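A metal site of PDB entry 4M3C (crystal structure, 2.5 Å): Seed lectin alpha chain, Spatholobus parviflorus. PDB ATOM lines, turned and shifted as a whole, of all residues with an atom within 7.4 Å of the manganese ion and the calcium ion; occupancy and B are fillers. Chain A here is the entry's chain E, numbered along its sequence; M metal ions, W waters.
Water W2 binds the calcium ion (2.0 Å). The calcium ion is bound by OD2 of Asp 137. The calcium ion is bound by water W4. The backbone carbonyl oxygen (O) of Tyr 130 binds the calcium ion (2.4 Å). OD2 of Asp 128 is bound to the calcium ion. The side-chain amide nitrogen (ND2) of Asn 132 binds the calcium ion (2.6 Å). The calcium ion is bound by OD1 of Asp 128 (2.8 Å).
ND1 of His 142 is in hydrogen-bond range of O of Tyr 140 (2.7 Å). OE1 of Glu 126 lies close to OD2 of Asp 146 (2.7 Å). The side-chain hydroxyl of Ser 152 lies close to the side-chain carboxylate of Glu 126 (3.2 Å). ND2 of Asn 132 sits close to OD2 of Asp 88 (3.4 Å). The backbone carbonyl oxygen (O) of Gly 144 sits at hydrogen-bond distance from the backbone NH (N) of Glu 126 (3.0 Å).
Within 4 Å of the calcium ion: Asp 128, Tyr 130, Asn 132 and Asp 137. The nearest printed residue that does not touch the calcium ion is Asp 88 (4.4 Å).
The manganese ion is bound by OD1 of Asp 128 (1.9 Å), water W3 (2.2 Å), water W1 (2.4 Å), OD1 of Asp 137 (2.4 Å), OE2 of Glu 126 (2.6 Å) and NE2 of His 142 (2.6 Å).
Water W1 lies within hydrogen-bond range of OE1 of Glu 126 (2.7 Å) and O of Ile 150 (2.7 Å).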
ATOM      1  N   ASP A  88      35.112  -1.298 -13.321  1.00  0.00           N
ATOM      2  CA  ASP A  88      34.029  -1.766 -14.196  1.00  0.00           C
ATOM      3  C   ASP A  88      32.886  -2.449 -13.430  1.00  0.00           C
ATOM      4  O   ASP A  88      31.798  -2.618 -14.004  1.00  0.00           O
ATOM      5  CB  ASP A  88      34.540  -2.744 -15.257  1.00  0.00           C
ATOM      6  CG  ASP A  88      35.161  -2.054 -16.448  1.00  0.00           C
ATOM      7  OD1 ASP A  88      36.259  -1.506 -16.300  1.00  0.00           O
ATOM      8  OD2 ASP A  88      34.562  -2.091 -17.537  1.00  0.00           O
ATOM      9  N   GLY A  89      33.136  -2.838 -12.173  1.00  0.00           N
ATOM     10  CA  GLY A  89      32.188  -3.590 -11.398  1.00  0.00           C
ATOM     11  C   GLY A  89      32.734  -4.767 -10.582  1.00  0.00           C
ATOM     12  O   GLY A  89      33.946  -5.045 -10.522  1.00  0.00           O
ATOM     13  N   GLY A 105      39.188  -5.793 -16.741  1.00  0.00           N
ATOM     14  CA  GLY A 105      38.379  -4.664 -17.229  1.00  0.00           C
ATOM     15  C   GLY A 105      36.894  -4.991 -17.161  1.00  0.00           C
ATOM     16  O   GLY A 105      36.399  -5.485 -16.148  1.00  0.00           O
ATOM     17  N   GLY A 106      36.191  -4.775 -18.273  1.00  0.00           N
ATOM     18  CA  GLY A 106      34.750  -5.035 -18.366  1.00  0.00           C
ATOM     19  C   GLY A 106      34.310  -6.484 -18.409  1.00  0.00           C
ATOM     20  O   GLY A 106      33.107  -6.781 -18.532  1.00  0.00           O
ATOM     21  N   PHE A 107      35.259  -7.386 -18.283  1.00  0.00           N
ATOM     22  CA  PHE A 107      34.969  -8.819 -18.347  1.00  0.00           C
ATOM     23  C   PHE A 107      34.799  -9.296 -16.907  1.00  0.00           C
ATOM     24  O   PHE A 107      34.260 -10.374 -16.681  1.00  0.00           O
ATOM     25  CB  PHE A 107      36.093  -9.622 -19.067  1.00  0.00           C
ATOM     26  CG  PHE A 107      36.435  -9.116 -20.464  1.00  0.00           C
ATOM     27  CD1 PHE A 107      35.719  -9.533 -21.574  1.00  0.00           C
ATOM     28  CD2 PHE A 107      37.491  -8.214 -20.659  1.00  0.00           C
ATOM     29  CE1 PHE A 107      36.021  -9.050 -22.838  1.00  0.00           C
ATOM     30  CE2 PHE A 107      37.808  -7.734 -21.915  1.00  0.00           C
ATOM     31  CZ  PHE A 107      37.067  -8.154 -23.005  1.00  0.00           C
ATOM     32  N   LEU A 108      35.282  -8.492 -15.944  1.00  0.00           N
ATOM     33  CA  LEU A 108      35.057  -8.734 -14.513  1.00  0.00           C
ATOM     34  C   LEU A 108      35.667 -10.049 -14.001  1.00  0.00           C
ATOM     35  O   LEU A 108      35.224 -10.590 -12.980  1.00  0.00           O
ATOM     36  CB  LEU A 108      33.544  -8.683 -14.170  1.00  0.00           C
ATOM     37  CG  LEU A 108      32.642  -7.599 -14.809  1.00  0.00           C
ATOM     38  CD1 LEU A 108      31.150  -7.844 -14.529  1.00  0.00           C
ATOM     39  CD2 LEU A 108      33.055  -6.191 -14.374  1.00  0.00           C
ATOM     40  N   GLU A 126      26.037  -9.679 -11.553  1.00  0.00           N
ATOM     41  CA  GLU A 126      27.000  -8.615 -11.624  1.00  0.00           C
ATOM     42  C   GLU A 126      26.354  -7.278 -11.233  1.00  0.00           C
ATOM     43  O   GLU A 126      25.146  -7.066 -11.401  1.00  0.00           O
ATOM     44  CB  GLU A 126      27.526  -8.518 -13.060  1.00  0.00           C
ATOM     45  CG  GLU A 126      26.386  -8.389 -14.069  1.00  0.00           C
ATOM     46  CD  GLU A 126      26.825  -7.706 -15.373  1.00  0.00           C
ATOM     47  OE1 GLU A 126      27.908  -8.057 -15.917  1.00  0.00           O
ATOM     48  OE2 GLU A 126      26.085  -6.822 -15.868  1.00  0.00           O
ATOM     49  N   PHE A 127      27.212  -6.393 -10.771  1.00  0.00           N
ATOM     50  CA  PHE A 127      26.831  -5.069 -10.317  1.00  0.00           C
ATOM     51  C   PHE A 127      27.842  -4.280 -11.092  1.00  0.00           C
ATOM     52  O   PHE A 127      28.986  -4.097 -10.683  1.00  0.00           O
ATOM     53  CB  PHE A 127      26.993  -4.938  -8.796  1.00  0.00           C
ATOM     54  CG  PHE A 127      26.219  -5.963  -8.011  1.00  0.00           C
ATOM     55  CD1 PHE A 127      24.870  -5.768  -7.705  1.00  0.00           C
ATOM     56  CD2 PHE A 127      26.805  -7.142  -7.617  1.00  0.00           C
ATOM     57  CE1 PHE A 127      24.136  -6.708  -7.004  1.00  0.00           C
ATOM     58  CE2 PHE A 127      26.074  -8.098  -6.904  1.00  0.00           C
ATOM     59  CZ  PHE A 127      24.739  -7.877  -6.601  1.00  0.00           C
ATOM     60  N   ASP A 128      27.355  -3.864 -12.266  1.00  0.00           N
ATOM     61  CA  ASP A 128      28.154  -3.395 -13.362  1.00  0.00           C
ATOM     62  C   ASP A 128      28.154  -1.884 -13.387  1.00  0.00           C
ATOM     63  O   ASP A 128      27.120  -1.215 -13.447  1.00  0.00           O
ATOM     64  CB  ASP A 128      27.528  -3.971 -14.625  1.00  0.00           C
ATOM     65  CG  ASP A 128      28.337  -3.697 -15.866  1.00  0.00           C
ATOM     66  OD1 ASP A 128      28.013  -4.342 -16.879  1.00  0.00           O
ATOM     67  OD2 ASP A 128      29.281  -2.873 -15.848  1.00  0.00           O
ATOM     68  N   THR A 129      29.337  -1.335 -13.413  1.00  0.00           N
ATOM     69  CA  THR A 129      29.513   0.030 -13.054  1.00  0.00           C
ATOM     70  C   THR A 129      29.932   0.885 -14.275  1.00  0.00           C
ATOM     71  O   THR A 129      30.001   2.116 -14.203  1.00  0.00           O
ATOM     72  CB  THR A 129      30.430   0.017 -11.829  1.00  0.00           C
ATOM     73  OG1 THR A 129      29.825   0.716 -10.729  1.00  0.00           O
ATOM     74  CG2 THR A 129      31.826   0.455 -12.114  1.00  0.00           C
ATOM     75  N   TYR A 130      30.117   0.243 -15.423  1.00  0.00           N
ATOM     76  CA  TYR A 130      30.545   0.942 -16.618  1.00  0.00           C
ATOM     77  C   TYR A 130      29.818   0.414 -17.873  1.00  0.00           C
ATOM     78  O   TYR A 130      29.803  -0.795 -18.117  1.00  0.00           O
ATOM     79  CB  TYR A 130      32.062   0.807 -16.787  1.00  0.00           C
ATOM     80  CG  TYR A 130      32.562   1.420 -18.084  1.00  0.00           C
ATOM     81  CD1 TYR A 130      33.090   2.711 -18.106  1.00  0.00           C
ATOM     82  CD2 TYR A 130      32.485   0.732 -19.290  1.00  0.00           C
ATOM     83  CE1 TYR A 130      33.556   3.286 -19.274  1.00  0.00           C
ATOM     84  CE2 TYR A 130      32.934   1.296 -20.467  1.00  0.00           C
ATOM     85  CZ  TYR A 130      33.485   2.574 -20.463  1.00  0.00           C
ATOM     86  OH  TYR A 130      33.940   3.159 -21.633  1.00  0.00           O
ATOM     87  N   GLU A 131      29.234   1.316 -18.674  1.00  0.00           N
ATOM     88  CA  GLU A 131      28.550   0.915 -19.906  1.00  0.00           C
ATOM     89  C   GLU A 131      29.509   0.541 -21.059  1.00  0.00           C
ATOM     90  O   GLU A 131      30.115   1.417 -21.725  1.00  0.00           O
ATOM     91  CB  GLU A 131      27.515   1.956 -20.365  1.00  0.00           C
ATOM     92  CG  GLU A 131      26.618   1.431 -21.485  1.00  0.00           C
ATOM     93  CD  GLU A 131      25.847   2.491 -22.261  1.00  0.00           C
ATOM     94  OE1 GLU A 131      26.053   3.702 -22.067  1.00  0.00           O
ATOM     95  OE2 GLU A 131      25.000   2.111 -23.099  1.00  0.00           O
ATOM     96  N   ASN A 132      29.629  -0.769 -21.270  1.00  0.00           N
ATOM     97  CA  ASN A 132      30.340  -1.312 -22.412  1.00  0.00           C
ATOM     98  C   ASN A 132      29.292  -1.653 -23.465  1.00  0.00           C
ATOM     99  O   ASN A 132      28.655  -2.703 -23.378  1.00  0.00           O
ATOM    100  CB  ASN A 132      31.091  -2.591 -21.992  1.00  0.00           C
ATOM    101  CG  ASN A 132      32.262  -2.325 -21.055  1.00  0.00           C
ATOM    102  OD1 ASN A 132      33.413  -2.314 -21.488  1.00  0.00           O
ATOM    103  ND2 ASN A 132      31.979  -2.112 -19.778  1.00  0.00           N
ATOM    104  N   THR A 133      29.095  -0.744 -24.445  1.00  0.00           N
ATOM    105  CA  THR A 133      28.105  -0.928 -25.525  1.00  0.00           C
ATOM    106  C   THR A 133      28.523  -2.128 -26.332  1.00  0.00           C
ATOM    107  O   THR A 133      27.719  -2.743 -27.006  1.00  0.00           O
ATOM    108  CB  THR A 133      27.911   0.284 -26.507  1.00  0.00           C
ATOM    109  OG1 THR A 133      29.149   0.985 -26.700  1.00  0.00           O
ATOM    110  CG2 THR A 133      26.827   1.262 -26.038  1.00  0.00           C
ATOM    111  N   PHE A 135      29.040  -4.855 -25.011  1.00  0.00           N
ATOM    112  CA  PHE A 135      28.470  -6.021 -24.335  1.00  0.00           C
ATOM    113  C   PHE A 135      26.962  -5.885 -24.217  1.00  0.00           C
ATOM    114  O   PHE A 135      26.311  -6.579 -23.430  1.00  0.00           O
ATOM    115  CB  PHE A 135      29.102  -6.198 -22.947  1.00  0.00           C
ATOM    116  CG  PHE A 135      30.611  -6.335 -22.948  1.00  0.00           C
ATOM    117  CD1 PHE A 135      31.310  -6.775 -24.083  1.00  0.00           C
ATOM    118  CD2 PHE A 135      31.339  -6.081 -21.807  1.00  0.00           C
ATOM    119  CE1 PHE A 135      32.691  -6.925 -24.066  1.00  0.00           C
ATOM    120  CE2 PHE A 135      32.709  -6.230 -21.768  1.00  0.00           C
ATOM    121  CZ  PHE A 135      33.395  -6.639 -22.892  1.00  0.00           C
ATOM    122  N   THR A 136      26.400  -5.015 -25.033  1.00  0.00           N
ATOM    123  CA  THR A 136      25.033  -4.506 -24.844  1.00  0.00           C
ATOM    124  C   THR A 136      24.754  -4.097 -23.373  1.00  0.00           C
ATOM    125  O   THR A 136      23.691  -4.415 -22.816  1.00  0.00           O
ATOM    126  CB  THR A 136      23.928  -5.402 -25.507  1.00  0.00           C
ATOM    127  OG1 THR A 136      24.446  -6.087 -26.651  1.00  0.00           O
ATOM    128  CG2 THR A 136      22.711  -4.542 -25.956  1.00  0.00           C
ATOM    129  N   ASP A 137      25.708  -3.378 -22.753  1.00  0.00           N
ATOM    130  CA  ASP A 137      25.412  -2.679 -21.482  1.00  0.00           C
ATOM    131  C   ASP A 137      24.385  -1.585 -21.668  1.00  0.00           C
ATOM    132  O   ASP A 137      24.507  -0.791 -22.603  1.00  0.00           O
ATOM    133  CB  ASP A 137      26.639  -2.087 -20.836  1.00  0.00           C
ATOM    134  CG  ASP A 137      27.415  -3.103 -20.087  1.00  0.00           C
ATOM    135  OD1 ASP A 137      26.891  -4.219 -20.000  1.00  0.00           O
ATOM    136  OD2 ASP A 137      28.516  -2.832 -19.566  1.00  0.00           O
ATOM    137  N   PRO A 138      23.361  -1.570 -20.778  1.00  0.00           N
ATOM    138  CA  PRO A 138      22.398  -0.496 -20.737  1.00  0.00           C
ATOM    139  C   PRO A 138      23.097   0.731 -20.163  1.00  0.00           C
ATOM    140  O   PRO A 138      24.151   0.576 -19.505  1.00  0.00           O
ATOM    141  CB  PRO A 138      21.299  -1.013 -19.776  1.00  0.00           C
ATOM    142  CG  PRO A 138      21.778  -2.305 -19.216  1.00  0.00           C
ATOM    143  CD  PRO A 138      23.208  -2.494 -19.637  1.00  0.00           C
ATOM    144  N   TYR A 140      22.728   2.959 -17.723  1.00  0.00           N
ATOM    145  CA  TYR A 140      22.904   3.298 -16.334  1.00  0.00           C
ATOM    146  C   TYR A 140      23.632   2.178 -15.626  1.00  0.00           C
ATOM    147  O   TYR A 140      23.657   1.062 -16.094  1.00  0.00           O
ATOM    148  CB  TYR A 140      21.539   3.531 -15.684  1.00  0.00           C
ATOM    149  CG  TYR A 140      20.485   2.587 -16.205  1.00  0.00           C
ATOM    150  CD1 TYR A 140      20.443   1.263 -15.800  1.00  0.00           C
ATOM    151  CD2 TYR A 140      19.537   3.020 -17.130  1.00  0.00           C
ATOM    152  CE1 TYR A 140      19.477   0.393 -16.280  1.00  0.00           C
ATOM    153  CE2 TYR A 140      18.559   2.167 -17.617  1.00  0.00           C
ATOM    154  CZ  TYR A 140      18.530   0.861 -17.192  1.00  0.00           C
ATOM    155  OH  TYR A 140      17.581   0.012 -17.716  1.00  0.00           O
ATOM    156  N   HIS A 142      23.884  -0.847 -13.345  1.00  0.00           N
ATOM    157  CA  HIS A 142      22.861  -1.927 -13.413  1.00  0.00           C
ATOM    158  C   HIS A 142      23.264  -3.195 -12.766  1.00  0.00           C
ATOM    159  O   HIS A 142      24.437  -3.447 -12.541  1.00  0.00           O
ATOM    160  CB  HIS A 142      22.510  -2.214 -14.854  1.00  0.00           C
ATOM    161  CG  HIS A 142      23.710  -2.509 -15.728  1.00  0.00           C
ATOM    162  ND1 HIS A 142      24.426  -1.542 -16.338  1.00  0.00           N
ATOM    163  CD2 HIS A 142      24.338  -3.708 -16.066  1.00  0.00           C
ATOM    164  CE1 HIS A 142      25.439  -2.080 -17.028  1.00  0.00           C
ATOM    165  NE2 HIS A 142      25.389  -3.401 -16.871  1.00  0.00           N
ATOM    166  N   ILE A 143      22.257  -4.000 -12.437  1.00  0.00           N
ATOM    167  CA  ILE A 143      22.438  -5.355 -11.912  1.00  0.00           C
ATOM    168  C   ILE A 143      22.171  -6.184 -13.138  1.00  0.00           C
ATOM    169  O   ILE A 143      21.410  -5.765 -13.978  1.00  0.00           O
ATOM    170  CB  ILE A 143      21.368  -5.669 -10.823  1.00  0.00           C
ATOM    171  CG1 ILE A 143      21.564  -4.759  -9.607  1.00  0.00           C
ATOM    172  CG2 ILE A 143      21.418  -7.137 -10.365  1.00  0.00           C
ATOM    173  CD1 ILE A 143      20.420  -4.786  -8.604  1.00  0.00           C
ATOM    174  N   GLY A 144      22.785  -7.360 -13.237  1.00  0.00           N
ATOM    175  CA  GLY A 144      22.609  -8.196 -14.411  1.00  0.00           C
ATOM    176  C   GLY A 144      22.802  -9.669 -14.100  1.00  0.00           C
ATOM    177  O   GLY A 144      23.565 -10.038 -13.158  1.00  0.00           O
ATOM    178  N   ASP A 146      24.312 -12.920 -15.664  1.00  0.00           N
ATOM    179  CA  ASP A 146      25.273 -13.390 -16.690  1.00  0.00           C
ATOM    180  C   ASP A 146      25.247 -14.917 -16.781  1.00  0.00           C
ATOM    181  O   ASP A 146      25.552 -15.610 -15.794  1.00  0.00           O
ATOM    182  CB  ASP A 146      26.668 -12.876 -16.363  1.00  0.00           C
ATOM    183  CG  ASP A 146      26.730 -11.346 -16.430  1.00  0.00           C
ATOM    184  OD1 ASP A 146      25.694 -10.742 -16.814  1.00  0.00           O
ATOM    185  OD2 ASP A 146      27.808 -10.740 -16.114  1.00  0.00           O
ATOM    186  N   ILE A 150      28.895 -12.335 -20.833  1.00  0.00           N
ATOM    187  CA  ILE A 150      28.819 -11.016 -20.215  1.00  0.00           C
ATOM    188  C   ILE A 150      27.650 -10.184 -20.832  1.00  0.00           C
ATOM    189  O   ILE A 150      27.209  -9.174 -20.257  1.00  0.00           O
ATOM    190  CB  ILE A 150      30.176 -10.305 -20.375  1.00  0.00           C
ATOM    191  CG1 ILE A 150      30.288  -9.071 -19.463  1.00  0.00           C
ATOM    192  CG2 ILE A 150      30.446 -10.006 -21.826  1.00  0.00           C
ATOM    193  CD1 ILE A 150      30.966  -9.367 -18.147  1.00  0.00           C
ATOM    194  N   SER A 151      27.106 -10.596 -21.982  1.00  0.00           N
ATOM    195  CA  SER A 151      25.922  -9.907 -22.465  1.00  0.00           C
ATOM    196  C   SER A 151      24.764 -10.434 -21.620  1.00  0.00           C
ATOM    197  O   SER A 151      24.180 -11.483 -21.952  1.00  0.00           O
ATOM    198  CB  SER A 151      25.638 -10.161 -23.964  1.00  0.00           C
ATOM    199  OG  SER A 151      26.450  -9.349 -24.807  1.00  0.00           O
ATOM    200  N   SER A 152      24.477  -9.711 -20.523  1.00  0.00           N
ATOM    201  CA  SER A 152      23.485 -10.136 -19.535  1.00  0.00           C
ATOM    202  C   SER A 152      22.170 -10.537 -20.173  1.00  0.00           C
ATOM    203  O   SER A 152      21.613  -9.839 -21.034  1.00  0.00           O
ATOM    204  CB  SER A 152      23.232  -9.033 -18.496  1.00  0.00           C
ATOM    205  OG  SER A 152      24.435  -8.622 -17.883  1.00  0.00           O
ATOM    206  N   THR A 155      18.733  -7.341 -17.261  1.00  0.00           N
ATOM    207  CA  THR A 155      19.200  -6.288 -16.298  1.00  0.00           C
ATOM    208  C   THR A 155      18.072  -5.391 -15.687  1.00  0.00           C
ATOM    209  O   THR A 155      16.965  -5.392 -16.219  1.00  0.00           O
ATOM    210  CB  THR A 155      20.198  -5.323 -16.953  1.00  0.00           C
ATOM    211  OG1 THR A 155      19.544  -4.620 -18.036  1.00  0.00           O
ATOM    212  CG2 THR A 155      21.467  -6.102 -17.477  1.00  0.00           C
HETATM  213 MN    MN M   1      26.759  -5.334 -17.835  1.00  0.00          MN
HETATM  214 CA    CA M   2      30.248  -3.186 -18.105  1.00  0.00          CA
HETATM  215  O   HOH W   1      27.944  -7.281 -18.461  1.00  0.00           O
HETATM  216  O   HOH W   2      31.873  -2.808 -16.922  1.00  0.00           O
HETATM  217  O   HOH W   3      24.916  -6.400 -18.543  1.00  0.00           O
HETATM  218  O   HOH W   4      30.427  -5.507 -18.383  1.00  0.00           O
